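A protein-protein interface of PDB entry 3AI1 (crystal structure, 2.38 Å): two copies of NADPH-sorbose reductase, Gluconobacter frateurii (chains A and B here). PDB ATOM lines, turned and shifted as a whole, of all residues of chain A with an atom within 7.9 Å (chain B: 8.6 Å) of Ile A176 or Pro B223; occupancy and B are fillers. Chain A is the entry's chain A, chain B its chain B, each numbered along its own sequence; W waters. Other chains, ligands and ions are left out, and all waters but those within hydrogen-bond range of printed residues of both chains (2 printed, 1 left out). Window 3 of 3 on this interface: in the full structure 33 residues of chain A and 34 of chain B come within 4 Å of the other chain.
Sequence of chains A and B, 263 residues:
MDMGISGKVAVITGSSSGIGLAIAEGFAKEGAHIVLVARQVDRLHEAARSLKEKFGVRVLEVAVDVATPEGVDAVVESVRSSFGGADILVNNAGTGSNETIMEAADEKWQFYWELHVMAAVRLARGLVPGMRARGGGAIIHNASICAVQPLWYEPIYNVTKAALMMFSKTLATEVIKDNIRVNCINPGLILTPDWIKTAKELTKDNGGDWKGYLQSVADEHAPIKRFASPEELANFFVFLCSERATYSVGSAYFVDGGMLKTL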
ATOM      1  N   GLY A 137     -28.195 -40.793  17.462  1.00  0.00           N
ATOM      2  CA  GLY A 137     -28.231 -40.776  16.003  1.00  0.00           C
ATOM      3  C   GLY A 137     -27.975 -39.424  15.361  1.00  0.00           C
ATOM      4  O   GLY A 137     -27.315 -38.565  15.939  1.00  0.00           O
ATOM      5  N   LYS A 169     -31.528 -25.673  14.416  1.00  0.00           N
ATOM      6  CA  LYS A 169     -30.587 -25.273  15.461  1.00  0.00           C
ATOM      7  C   LYS A 169     -31.164 -25.361  16.871  1.00  0.00           C
ATOM      8  O   LYS A 169     -30.440 -25.667  17.818  1.00  0.00           O
ATOM      9  CB  LYS A 169     -30.010 -23.873  15.215  1.00  0.00           C
ATOM     10  CG  LYS A 169     -28.835 -23.561  16.156  1.00  0.00           C
ATOM     11  CD  LYS A 169     -28.039 -22.347  15.728  1.00  0.00           C
ATOM     12  CE  LYS A 169     -26.865 -22.114  16.677  1.00  0.00           C
ATOM     13  NZ  LYS A 169     -25.789 -23.149  16.516  1.00  0.00           N
ATOM     14  N   THR A 170     -32.456 -25.080  17.018  1.00  0.00           N
ATOM     15  CA  THR A 170     -33.096 -25.204  18.329  1.00  0.00           C
ATOM     16  C   THR A 170     -33.211 -26.678  18.742  1.00  0.00           C
ATOM     17  O   THR A 170     -33.043 -27.007  19.914  1.00  0.00           O
ATOM     18  CB  THR A 170     -34.479 -24.524  18.393  1.00  0.00           C
ATOM     19  OG1 THR A 170     -35.350 -25.114  17.418  1.00  0.00           O
ATOM     20  CG2 THR A 170     -34.365 -23.030  18.145  1.00  0.00           C
ATOM     21  N   LEU A 171     -33.487 -27.555  17.783  1.00  0.00           N
ATOM     22  CA  LEU A 171     -33.562 -28.990  18.054  1.00  0.00           C
ATOM     23  C   LEU A 171     -32.185 -29.521  18.431  1.00  0.00           C
ATOM     24  O   LEU A 171     -32.052 -30.277  19.393  1.00  0.00           O
ATOM     25  CB  LEU A 171     -34.138 -29.757  16.857  1.00  0.00           C
ATOM     26  CG  LEU A 171     -34.438 -31.251  17.066  1.00  0.00           C
ATOM     27  CD1 LEU A 171     -35.630 -31.479  18.008  1.00  0.00           C
ATOM     28  CD2 LEU A 171     -34.675 -31.955  15.736  1.00  0.00           C
ATOM     29  N   ALA A 172     -31.167 -29.089  17.686  1.00  0.00           N
ATOM     30  CA  ALA A 172     -29.778 -29.440  17.964  1.00  0.00           C
ATOM     31  C   ALA A 172     -29.377 -29.189  19.416  1.00  0.00           C
ATOM     32  O   ALA A 172     -28.761 -30.043  20.055  1.00  0.00           O
ATOM     33  CB  ALA A 172     -28.848 -28.701  17.030  1.00  0.00           C
ATOM     34  N   THR A 173     -29.737 -28.019  19.927  1.00  0.00           N
ATOM     35  CA  THR A 173     -29.403 -27.615  21.298  1.00  0.00           C
ATOM     36  C   THR A 173     -30.095 -28.499  22.342  1.00  0.00           C
ATOM     37  O   THR A 173     -29.537 -28.764  23.403  1.00  0.00           O
ATOM     38  CB  THR A 173     -29.747 -26.119  21.514  1.00  0.00           C
ATOM     39  OG1 THR A 173     -28.764 -25.319  20.847  1.00  0.00           O
ATOM     40  CG2 THR A 173     -29.759 -25.741  22.983  1.00  0.00           C
ATOM     41  N   GLU A 174     -31.295 -28.968  22.007  1.00  0.00           N
ATOM     42  CA  GLU A 174     -32.143 -29.706  22.933  1.00  0.00           C
ATOM     43  C   GLU A 174     -31.836 -31.212  22.995  1.00  0.00           C
ATOM     44  O   GLU A 174     -31.962 -31.832  24.053  1.00  0.00           O
ATOM     45  CB  GLU A 174     -33.609 -29.486  22.546  1.00  0.00           C
ATOM     46  CG  GLU A 174     -34.623 -29.960  23.582  1.00  0.00           C
ATOM     47  CD  GLU A 174     -36.061 -29.690  23.174  1.00  0.00           C
ATOM     48  OE1 GLU A 174     -36.883 -30.634  23.275  1.00  0.00           O
ATOM     49  OE2 GLU A 174     -36.368 -28.537  22.762  1.00  0.00           O
ATOM     50  N   VAL A 175     -31.442 -31.796  21.867  1.00  0.00           N
ATOM     51  CA  VAL A 175     -31.310 -33.249  21.773  1.00  0.00           C
ATOM     52  C   VAL A 175     -29.881 -33.791  21.755  1.00  0.00           C
ATOM     53  O   VAL A 175     -29.692 -35.005  21.798  1.00  0.00           O
ATOM     54  CB  VAL A 175     -32.112 -33.834  20.582  1.00  0.00           C
ATOM     55  CG1 VAL A 175     -33.600 -33.493  20.716  1.00  0.00           C
ATOM     56  CG2 VAL A 175     -31.548 -33.355  19.257  1.00  0.00           C
ATOM     57  N   ILE A 176     -28.884 -32.907  21.696  1.00  0.00           N
ATOM     58  CA  ILE A 176     -27.484 -33.335  21.796  1.00  0.00           C
ATOM     59  C   ILE A 176     -27.191 -34.060  23.123  1.00  0.00           C
ATOM     60  O   ILE A 176     -26.315 -34.929  23.182  1.00  0.00           O
ATOM     61  CB  ILE A 176     -26.459 -32.172  21.528  1.00  0.00           C
ATOM     62  CG1 ILE A 176     -25.029 -32.710  21.416  1.00  0.00           C
ATOM     63  CG2 ILE A 176     -26.547 -31.060  22.601  1.00  0.00           C
ATOM     64  CD1 ILE A 176     -24.822 -33.733  20.299  1.00  0.00           C
ATOM     65  N   LYS A 177     -27.949 -33.727  24.168  1.00  0.00           N
ATOM     66  CA  LYS A 177     -27.865 -34.452  25.438  1.00  0.00           C
ATOM     67  C   LYS A 177     -28.169 -35.958  25.302  1.00  0.00           C
ATOM     68  O   LYS A 177     -27.668 -36.758  26.083  1.00  0.00           O
ATOM     69  CB  LYS A 177     -28.747 -33.809  26.520  1.00  0.00           C
ATOM     70  CG  LYS A 177     -30.248 -33.819  26.245  1.00  0.00           C
ATOM     71  CD  LYS A 177     -31.021 -33.454  27.504  1.00  0.00           C
ATOM     72  CE  LYS A 177     -32.273 -32.635  27.208  1.00  0.00           C
ATOM     73  NZ  LYS A 177     -31.967 -31.173  27.035  1.00  0.00           N
ATOM     74  N   ASP A 178     -28.975 -36.322  24.304  1.00  0.00           N
ATOM     75  CA  ASP A 178     -29.333 -37.723  24.030  1.00  0.00           C
ATOM     76  C   ASP A 178     -28.428 -38.357  22.978  1.00  0.00           C
ATOM     77  O   ASP A 178     -28.787 -39.367  22.371  1.00  0.00           O
ATOM     78  CB  ASP A 178     -30.788 -37.813  23.550  1.00  0.00           C
ATOM     79  CG  ASP A 178     -31.785 -37.292  24.573  1.00  0.00           C
ATOM     80  OD1 ASP A 178     -31.526 -37.411  25.796  1.00  0.00           O
ATOM     81  OD2 ASP A 178     -32.841 -36.772  24.142  1.00  0.00           O
ATOM     82  N   ASN A 179     -27.260 -37.748  22.768  1.00  0.00           N
ATOM     83  CA  ASN A 179     -26.318 -38.153  21.731  1.00  0.00           C
ATOM     84  C   ASN A 179     -26.939 -38.135  20.328  1.00  0.00           C
ATOM     85  O   ASN A 179     -26.707 -39.033  19.513  1.00  0.00           O
ATOM     86  CB  ASN A 179     -25.682 -39.519  22.055  1.00  0.00           C
ATOM     87  CG  ASN A 179     -24.409 -39.768  21.267  1.00  0.00           C
ATOM     88  OD1 ASN A 179     -23.665 -38.833  20.962  1.00  0.00           O
ATOM     89  ND2 ASN A 179     -24.159 -41.023  20.921  1.00  0.00           N
ATOM     90  N   ILE A 180     -27.734 -37.104  20.056  1.00  0.00           N
ATOM     91  CA  ILE A 180     -28.338 -36.926  18.736  1.00  0.00           C
ATOM     92  C   ILE A 180     -27.823 -35.637  18.096  1.00  0.00           C
ATOM     93  O   ILE A 180     -28.030 -34.545  18.625  1.00  0.00           O
ATOM     94  CB  ILE A 180     -29.896 -36.947  18.784  1.00  0.00           C
ATOM     95  CG1 ILE A 180     -30.395 -38.256  19.410  1.00  0.00           C
ATOM     96  CG2 ILE A 180     -30.483 -36.768  17.375  1.00  0.00           C
ATOM     97  CD1 ILE A 180     -31.886 -38.291  19.743  1.00  0.00           C
ATOM     98  N   ARG A 181     -27.143 -35.777  16.961  1.00  0.00           N
ATOM     99  CA  ARG A 181     -26.590 -34.619  16.251  1.00  0.00           C
ATOM    100  C   ARG A 181     -27.579 -34.108  15.226  1.00  0.00           C
ATOM    101  O   ARG A 181     -28.048 -34.866  14.380  1.00  0.00           O
ATOM    102  CB  ARG A 181     -25.286 -34.968  15.549  1.00  0.00           C
ATOM    103  CG  ARG A 181     -24.129 -35.285  16.465  1.00  0.00           C
ATOM    104  CD  ARG A 181     -23.419 -36.540  15.970  1.00  0.00           C
ATOM    105  NE  ARG A 181     -23.294 -36.563  14.510  1.00  0.00           N
ATOM    106  CZ  ARG A 181     -23.222 -37.673  13.783  1.00  0.00           C
ATOM    107  NH1 ARG A 181     -23.275 -38.869  14.371  1.00  0.00           N
ATOM    108  NH2 ARG A 181     -23.101 -37.590  12.464  1.00  0.00           N
ATOM    109  N   VAL A 182     -27.906 -32.824  15.309  1.00  0.00           N
ATOM    110  CA  VAL A 182     -28.816 -32.223  14.341  1.00  0.00           C
ATOM    111  C   VAL A 182     -28.092 -31.159  13.539  1.00  0.00           C
ATOM    112  O   VAL A 182     -27.475 -30.255  14.094  1.00  0.00           O
ATOM    113  CB  VAL A 182     -30.096 -31.658  14.994  1.00  0.00           C
ATOM    114  CG1 VAL A 182     -31.028 -31.105  13.936  1.00  0.00           C
ATOM    115  CG2 VAL A 182     -30.808 -32.739  15.807  1.00  0.00           C
ATOM    116  N   THR A 246     -18.935 -36.493  13.888  1.00  0.00           N
ATOM    117  CA  THR A 246     -19.409 -36.545  15.277  1.00  0.00           C
ATOM    118  C   THR A 246     -19.344 -35.227  16.056  1.00  0.00           C
ATOM    119  O   THR A 246     -19.871 -35.147  17.167  1.00  0.00           O
ATOM    120  CB  THR A 246     -18.648 -37.631  16.081  1.00  0.00           C
ATOM    121  OG1 THR A 246     -17.236 -37.506  15.846  1.00  0.00           O
ATOM    122  CG2 THR A 246     -19.093 -39.019  15.668  1.00  0.00           C
ATOM    123  N   TYR A 247     -18.694 -34.206  15.493  1.00  0.00           N
ATOM    124  CA  TYR A 247     -18.608 -32.915  16.169  1.00  0.00           C
ATOM    125  C   TYR A 247     -19.485 -31.833  15.512  1.00  0.00           C
ATOM    126  O   TYR A 247     -19.507 -30.689  15.953  1.00  0.00           O
ATOM    127  CB  TYR A 247     -17.144 -32.455  16.340  1.00  0.00           C
ATOM    128  CG  TYR A 247     -16.909 -31.593  17.577  1.00  0.00           C
ATOM    129  CD1 TYR A 247     -17.032 -32.132  18.865  1.00  0.00           C
ATOM    130  CD2 TYR A 247     -16.555 -30.242  17.460  1.00  0.00           C
ATOM    131  CE1 TYR A 247     -16.815 -31.345  20.010  1.00  0.00           C
ATOM    132  CE2 TYR A 247     -16.339 -29.442  18.599  1.00  0.00           C
ATOM    133  CZ  TYR A 247     -16.477 -30.003  19.866  1.00  0.00           C
ATOM    134  OH  TYR A 247     -16.269 -29.231  20.990  1.00  0.00           O
ATOM    135  N   SER A 248     -20.232 -32.214  14.485  1.00  0.00           N
ATOM    136  CA  SER A 248     -21.176 -31.310  13.839  1.00  0.00           C
ATOM    137  C   SER A 248     -22.506 -31.297  14.583  1.00  0.00           C
ATOM    138  O   SER A 248     -23.256 -32.277  14.565  1.00  0.00           O
ATOM    139  CB  SER A 248     -21.380 -31.701  12.377  1.00  0.00           C
ATOM    140  OG  SER A 248     -20.214 -31.406  11.621  1.00  0.00           O
ATOM    141  N   VAL A 249     -22.779 -30.179  15.247  1.00  0.00           N
ATOM    142  CA  VAL A 249     -23.997 -30.018  16.038  1.00  0.00           C
ATOM    143  C   VAL A 249     -24.575 -28.617  15.819  1.00  0.00           C
ATOM    144  O   VAL A 249     -23.929 -27.621  16.142  1.00  0.00           O
ATOM    145  CB  VAL A 249     -23.742 -30.231  17.556  1.00  0.00           C
ATOM    146  CG1 VAL A 249     -25.054 -30.254  18.314  1.00  0.00           C
ATOM    147  CG2 VAL A 249     -22.977 -31.520  17.811  1.00  0.00           C
ATOM    148  N   GLY A 250     -25.788 -28.553  15.269  1.00  0.00           N
ATOM    149  CA  GLY A 250     -26.478 -27.288  15.051  1.00  0.00           C
ATOM    150  C   GLY A 250     -25.848 -26.378  14.020  1.00  0.00           C
ATOM    151  O   GLY A 250     -25.956 -25.154  14.116  1.00  0.00           O
ATOM    152  N   ILE B 145     -13.967 -20.524  14.837  1.00  0.00           N
ATOM    153  CA  ILE B 145     -15.260 -20.002  15.278  1.00  0.00           C
ATOM    154  C   ILE B 145     -15.135 -18.501  15.587  1.00  0.00           C
ATOM    155  O   ILE B 145     -16.092 -17.745  15.440  1.00  0.00           O
ATOM    156  CB  ILE B 145     -15.837 -20.804  16.478  1.00  0.00           C
ATOM    157  CG1 ILE B 145     -17.238 -20.300  16.833  1.00  0.00           C
ATOM    158  CG2 ILE B 145     -14.891 -20.769  17.682  1.00  0.00           C
ATOM    159  CD1 ILE B 145     -18.140 -21.371  17.346  1.00  0.00           C
ATOM    160  N   GLN B 149     -17.485 -15.381  15.651  1.00  0.00           N
ATOM    161  CA  GLN B 149     -17.888 -15.224  17.044  1.00  0.00           C
ATOM    162  C   GLN B 149     -16.653 -14.914  17.911  1.00  0.00           C
ATOM    163  O   GLN B 149     -15.999 -15.822  18.418  1.00  0.00           O
ATOM    164  CB  GLN B 149     -18.594 -16.499  17.513  1.00  0.00           C
ATOM    165  CG  GLN B 149     -19.115 -16.458  18.931  1.00  0.00           C
ATOM    166  CD  GLN B 149     -19.991 -17.652  19.261  1.00  0.00           C
ATOM    167  OE1 GLN B 149     -21.116 -17.776  18.758  1.00  0.00           O
ATOM    168  NE2 GLN B 149     -19.482 -18.541  20.111  1.00  0.00           N
ATOM    169  N   LEU B 189     -13.821 -25.876  19.828  1.00  0.00           N
ATOM    170  CA  LEU B 189     -12.857 -26.360  20.801  1.00  0.00           C
ATOM    171  C   LEU B 189     -12.259 -27.678  20.328  1.00  0.00           C
ATOM    172  O   LEU B 189     -12.940 -28.705  20.297  1.00  0.00           O
ATOM    173  CB  LEU B 189     -13.520 -26.539  22.172  1.00  0.00           C
ATOM    174  CG  LEU B 189     -14.156 -25.307  22.822  1.00  0.00           C
ATOM    175  CD1 LEU B 189     -15.097 -25.727  23.952  1.00  0.00           C
ATOM    176  CD2 LEU B 189     -13.088 -24.336  23.319  1.00  0.00           C
ATOM    177  N   VAL B 217     -14.374 -25.321  30.633  1.00  0.00           N
ATOM    178  CA  VAL B 217     -14.337 -24.539  29.396  1.00  0.00           C
ATOM    179  C   VAL B 217     -15.350 -25.093  28.382  1.00  0.00           C
ATOM    180  O   VAL B 217     -16.111 -24.331  27.778  1.00  0.00           O
ATOM    181  CB  VAL B 217     -12.914 -24.512  28.782  1.00  0.00           C
ATOM    182  CG1 VAL B 217     -12.920 -23.873  27.401  1.00  0.00           C
ATOM    183  CG2 VAL B 217     -11.941 -23.776  29.707  1.00  0.00           C
ATOM    184  N   ALA B 218     -15.357 -26.416  28.220  1.00  0.00           N
ATOM    185  CA  ALA B 218     -16.297 -27.109  27.338  1.00  0.00           C
ATOM    186  C   ALA B 218     -17.758 -26.969  27.792  1.00  0.00           C
ATOM    187  O   ALA B 218     -18.654 -26.786  26.964  1.00  0.00           O
ATOM    188  CB  ALA B 218     -15.909 -28.576  27.215  1.00  0.00           C
ATOM    189  N   ASP B 219     -17.982 -27.053  29.105  1.00  0.00           N
ATOM    190  CA  ASP B 219     -19.308 -26.876  29.717  1.00  0.00           C
ATOM    191  C   ASP B 219     -19.852 -25.471  29.503  1.00  0.00           C
ATOM    192  O   ASP B 219     -21.065 -25.278  29.397  1.00  0.00           O
ATOM    193  CB  ASP B 219     -19.246 -27.144  31.229  1.00  0.00           C
ATOM    194  CG  ASP B 219     -18.993 -28.608  31.568  1.00  0.00           C
ATOM    195  OD1 ASP B 219     -18.933 -29.451  30.650  1.00  0.00           O
ATOM    196  OD2 ASP B 219     -18.845 -28.918  32.770  1.00  0.00           O
ATOM    197  N   GLU B 220     -18.938 -24.503  29.460  1.00  0.00           N
ATOM    198  CA  GLU B 220     -19.251 -23.079  29.300  1.00  0.00           C
ATOM    199  C   GLU B 220     -19.608 -22.733  27.853  1.00  0.00           C
ATOM    200  O   GLU B 220     -20.537 -21.961  27.608  1.00  0.00           O
ATOM    201  CB  GLU B 220     -18.045 -22.243  29.745  1.00  0.00           C
ATOM    202  CG  GLU B 220     -18.190 -20.722  29.627  1.00  0.00           C
ATOM    203  CD  GLU B 220     -18.444 -20.047  30.967  1.00  0.00           C
ATOM    204  OE1 GLU B 220     -17.533 -19.338  31.464  1.00  0.00           O
ATOM    205  OE2 GLU B 220     -19.550 -20.237  31.531  1.00  0.00           O
ATOM    206  N   HIS B 221     -18.878 -23.318  26.903  1.00  0.00           N
ATOM    207  CA  HIS B 221     -18.919 -22.876  25.509  1.00  0.00           C
ATOM    208  C   HIS B 221     -19.642 -23.795  24.532  1.00  0.00           C
ATOM    209  O   HIS B 221     -20.239 -23.321  23.573  1.00  0.00           O
ATOM    210  CB  HIS B 221     -17.504 -22.608  25.004  1.00  0.00           C
ATOM    211  CG  HIS B 221     -16.892 -21.370  25.579  1.00  0.00           C
ATOM    212  ND1 HIS B 221     -15.864 -21.404  26.498  1.00  0.00           N
ATOM    213  CD2 HIS B 221     -17.172 -20.062  25.373  1.00  0.00           C
ATOM    214  CE1 HIS B 221     -15.532 -20.168  26.827  1.00  0.00           C
ATOM    215  NE2 HIS B 221     -16.313 -19.336  26.160  1.00  0.00           N
ATOM    216  N   ALA B 222     -19.568 -25.102  24.764  1.00  0.00           N
ATOM    217  CA  ALA B 222     -20.109 -26.083  23.823  1.00  0.00           C
ATOM    218  C   ALA B 222     -21.257 -26.901  24.424  1.00  0.00           C
ATOM    219  O   ALA B 222     -21.085 -27.517  25.473  1.00  0.00           O
ATOM    220  CB  ALA B 222     -18.998 -27.000  23.324  1.00  0.00           C
ATOM    221  N   PRO B 223     -22.432 -26.899  23.758  1.00  0.00           N
ATOM    222  CA  PRO B 223     -23.610 -27.699  24.128  1.00  0.00           C
ATOM    223  C   PRO B 223     -23.346 -29.205  24.156  1.00  0.00           C
ATOM    224  O   PRO B 223     -24.019 -29.917  24.895  1.00  0.00           O
ATOM    225  CB  PRO B 223     -24.615 -27.368  23.019  1.00  0.00           C
ATOM    226  CG  PRO B 223     -24.245 -26.003  22.597  1.00  0.00           C
ATOM    227  CD  PRO B 223     -22.750 -25.965  22.662  1.00  0.00           C
ATOM    228  N   ILE B 224     -22.392 -29.676  23.349  1.00  0.00           N
ATOM    229  CA  ILE B 224     -21.962 -31.083  23.366  1.00  0.00           C
ATOM    230  C   ILE B 224     -21.070 -31.393  24.590  1.00  0.00           C
ATOM    231  O   ILE B 224     -20.806 -32.556  24.904  1.00  0.00           O
ATOM    232  CB  ILE B 224     -21.261 -31.493  22.031  1.00  0.00           C
ATOM    233  CG1 ILE B 224     -21.294 -33.022  21.845  1.00  0.00           C
ATOM    234  CG2 ILE B 224     -19.833 -30.903  21.950  1.00  0.00           C
ATOM    235  CD1 ILE B 224     -20.733 -33.527  20.516  1.00  0.00           C
ATOM    236  N   LYS B 225     -20.612 -30.332  25.258  1.00  0.00           N
ATOM    237  CA  LYS B 225     -19.877 -30.404  26.530  1.00  0.00           C
ATOM    238  C   LYS B 225     -18.618 -31.272  26.485  1.00  0.00           C
ATOM    239  O   LYS B 225     -18.271 -31.940  27.466  1.00  0.00           O
ATOM    240  CB  LYS B 225     -20.811 -30.840  27.671  1.00  0.00           C
ATOM    241  CG  LYS B 225     -21.911 -29.841  28.002  1.00  0.00           C
ATOM    242  CD  LYS B 225     -23.036 -30.517  28.779  1.00  0.00           C
ATOM    243  CE  LYS B 225     -23.979 -29.493  29.396  1.00  0.00           C
ATOM    244  NZ  LYS B 225     -23.627 -29.201  30.811  1.00  0.00           N
ATOM    245  N   ARG B 226     -17.942 -31.252  25.340  1.00  0.00           N
ATOM    246  CA  ARG B 226     -16.601 -31.827  25.221  1.00  0.00           C
ATOM    247  C   ARG B 226     -15.795 -31.123  24.131  1.00  0.00           C
ATOM    248  O   ARG B 226     -16.362 -30.513  23.222  1.00  0.00           O
ATOM    249  CB  ARG B 226     -16.651 -33.346  24.972  1.00  0.00           C
ATOM    250  CG  ARG B 226     -17.363 -33.770  23.694  1.00  0.00           C
ATOM    251  CD  ARG B 226     -17.158 -35.258  23.416  1.00  0.00           C
ATOM    252  NE  ARG B 226     -17.685 -35.648  22.105  1.00  0.00           N
ATOM    253  CZ  ARG B 226     -17.036 -35.516  20.947  1.00  0.00           C
ATOM    254  NH1 ARG B 226     -15.815 -34.993  20.904  1.00  0.00           N
ATOM    255  NH2 ARG B 226     -17.616 -35.906  19.822  1.00  0.00           N
ATOM    256  N   ASP B 256     -17.972 -27.298  15.407  1.00  0.00           N
ATOM    257  CA  ASP B 256     -17.884 -26.595  16.685  1.00  0.00           C
ATOM    258  C   ASP B 256     -18.696 -27.201  17.838  1.00  0.00           C
ATOM    259  O   ASP B 256     -18.655 -26.692  18.961  1.00  0.00           O
ATOM    260  CB  ASP B 256     -18.242 -25.115  16.488  1.00  0.00           C
ATOM    261  CG  ASP B 256     -19.615 -24.916  15.844  1.00  0.00           C
ATOM    262  OD1 ASP B 256     -19.772 -23.924  15.108  1.00  0.00           O
ATOM    263  OD2 ASP B 256     -20.528 -25.742  16.066  1.00  0.00           O
ATOM    264  N   GLY B 257     -19.424 -28.284  17.562  1.00  0.00           N
ATOM    265  CA  GLY B 257     -20.198 -28.985  18.592  1.00  0.00           C
ATOM    266  C   GLY B 257     -21.264 -28.138  19.273  1.00  0.00           C
ATOM    267  O   GLY B 257     -21.573 -28.344  20.444  1.00  0.00           O
ATOM    268  N   GLY B 258     -21.819 -27.183  18.532  1.00  0.00           N
ATOM    269  CA  GLY B 258     -22.893 -26.343  19.041  1.00  0.00           C
ATOM    270  C   GLY B 258     -22.436 -24.980  19.516  1.00  0.00           C
ATOM    271  O   GLY B 258     -23.263 -24.119  19.825  1.00  0.00           O
ATOM    272  N   MET B 259     -21.120 -24.784  19.565  1.00  0.00           N
ATOM    273  CA  MET B 259     -20.518 -23.595  20.169  1.00  0.00           C
ATOM    274  C   MET B 259     -20.973 -22.286  19.525  1.00  0.00           C
ATOM    275  O   MET B 259     -21.086 -21.272  20.208  1.00  0.00           O
ATOM    276  CB  MET B 259     -18.988 -23.704  20.162  1.00  0.00           C
ATOM    277  CG  MET B 259     -18.261 -22.575  20.888  1.00  0.00           C
ATOM    278  SD  MET B 259     -16.469 -22.775  20.877  1.00  0.00           S
ATOM    279  CE  MET B 259     -15.964 -21.165  21.482  1.00  0.00           C
ATOM    280  N   LEU B 260     -21.236 -22.323  18.222  1.00  0.00           N
ATOM    281  CA  LEU B 260     -21.745 -21.166  17.488  1.00  0.00           C
ATOM    282  C   LEU B 260     -23.170 -20.905  17.950  1.00  0.00           C
ATOM    283  O   LEU B 260     -24.018 -21.796  17.911  1.00  0.00           O
ATOM    284  CB  LEU B 260     -21.680 -21.411  15.975  1.00  0.00           C
ATOM    285  CG  LEU B 260     -21.502 -20.307  14.908  1.00  0.00           C
ATOM    286  CD1 LEU B 260     -22.639 -20.285  13.884  1.00  0.00           C
ATOM    287  CD2 LEU B 260     -21.199 -18.896  15.446  1.00  0.00           C
ATOM    288  N   LYS B 261     -23.414 -19.685  18.412  1.00  0.00           N
ATOM    289  CA  LYS B 261     -24.659 -19.363  19.100  1.00  0.00           C
ATOM    290  C   LYS B 261     -25.664 -18.675  18.177  1.00  0.00           C
ATOM    291  O   LYS B 261     -26.795 -18.396  18.560  1.00  0.00           O
ATOM    292  CB  LYS B 261     -24.355 -18.553  20.370  1.00  0.00           C
ATOM    293  CG  LYS B 261     -23.959 -19.457  21.547  1.00  0.00           C
ATOM    294  CD  LYS B 261     -22.820 -18.886  22.377  1.00  0.00           C
ATOM    295  CE  LYS B 261     -22.357 -19.870  23.463  1.00  0.00           C
ATOM    296  NZ  LYS B 261     -21.477 -20.975  22.936  1.00  0.00           N
HETATM  297  O   HOH W   1     -16.467 -26.486  20.528  1.00  0.00           O
HETATM  298  O   HOH W   2     -20.697 -27.830  14.455  1.00  0.00           O
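Water W2 lies within hydrogen-bond range of OD2 of Asp B256, N of Val A249, N of Gly B257 and O of Tyr A247.
Water W1 lies within hydrogen-bond range of O of Asp B256, OH of Tyr A247, N of Leu B189 and SD of Met B259.
O of His B221 lies within hydrogen-bond range of NZ of Lys B261, 2.7 Å away.
O of Lys A169 is in hydrogen-bond range of OG1 of Thr A173 (3.5 Å).
O of Gly B257 sits at hydrogen-bond distance from N of Ile B224 (3.3 Å).
The side-chain amide oxygen (OE1) of Gln B149 sits at hydrogen-bond distance from the backbone NH (N) of Lys B261 (3.0 Å).
NZ of Lys B261 lies within hydrogen-bond range of O of Met B259 (2.8 Å).
OD2 of Asp B256 lies within hydrogen-bond range of N of Gly B258, 3.1 Å away.
The backbone carbonyl oxygen (O) of Leu B260 sits at hydrogen-bond distance from the side-chain amino group (NZ) of Lys A169, at 2.6 Å.
O of Arg B226 lies within hydrogen-bond range of OH of Tyr A247 (2.6 Å).
The backbone carbonyl oxygen (O) of Val A249 lies within hydrogen-bond range of the backbone NH (N) of Gly B258, 3.2 Å away.
The backbone carbonyl oxygen (O) of Tyr A247 lies within hydrogen-bond range of the backbone NH (N) of Gly B257 (2.9 Å).
OH of Tyr A247 sits at hydrogen-bond distance from O of Leu B189.
Among the printed residues, merely in contact across the chains: Tyr A247 with Asp B256, Thr A246 with Arg B226, Ile A176 with Pro B223, Tyr A247 with Ile B224, Val A249 with Gly B257, Ile A176 with Ile B224, Thr A246 with Ile B224, Val A249 with Asp B256 and Lys A169 with Lys B261.
No position is printed for both chains.
Of the 14 pairs that touch across the chains among the printed residues, none has its exchanged pair printed and touching as well.
Printed residues of chain B that touch a printed residue of chain A: Leu B189, Pro B223, Ile B224, Arg B226, Asp B256, Gly B257, Gly B258, Leu B260 and Lys B261.
Of the 20 printed residues of chain A, 5 touch a printed residue of chain B.
Pro B223 touches just one residue of chain A: Ile A176 (3.6 Å).
No residue of chain A comes within 4 Å of Ala B222.
Printed residues of chain A within 4 Å of Asp B256: Tyr A247 and Val A249.
Printed residues of chain A within 4 Å of Leu B260: Lys A169.
Of the printed residues of chain A, Gly B258 touches Val A249.
Of the printed residues of chain A, Ile B224 touches Ile A176, Thr A246 and Tyr A247.
The nearest residue of chain B that does not touch Ile A176 is Gly B257 (5.7 Å).
The nearest residue of chain A that does not touch Pro B223 is Thr A173 (4.9 Å).
The nearest printed residue of chain B that does not touch Val A249 is Ile B224 (4.05 Å).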
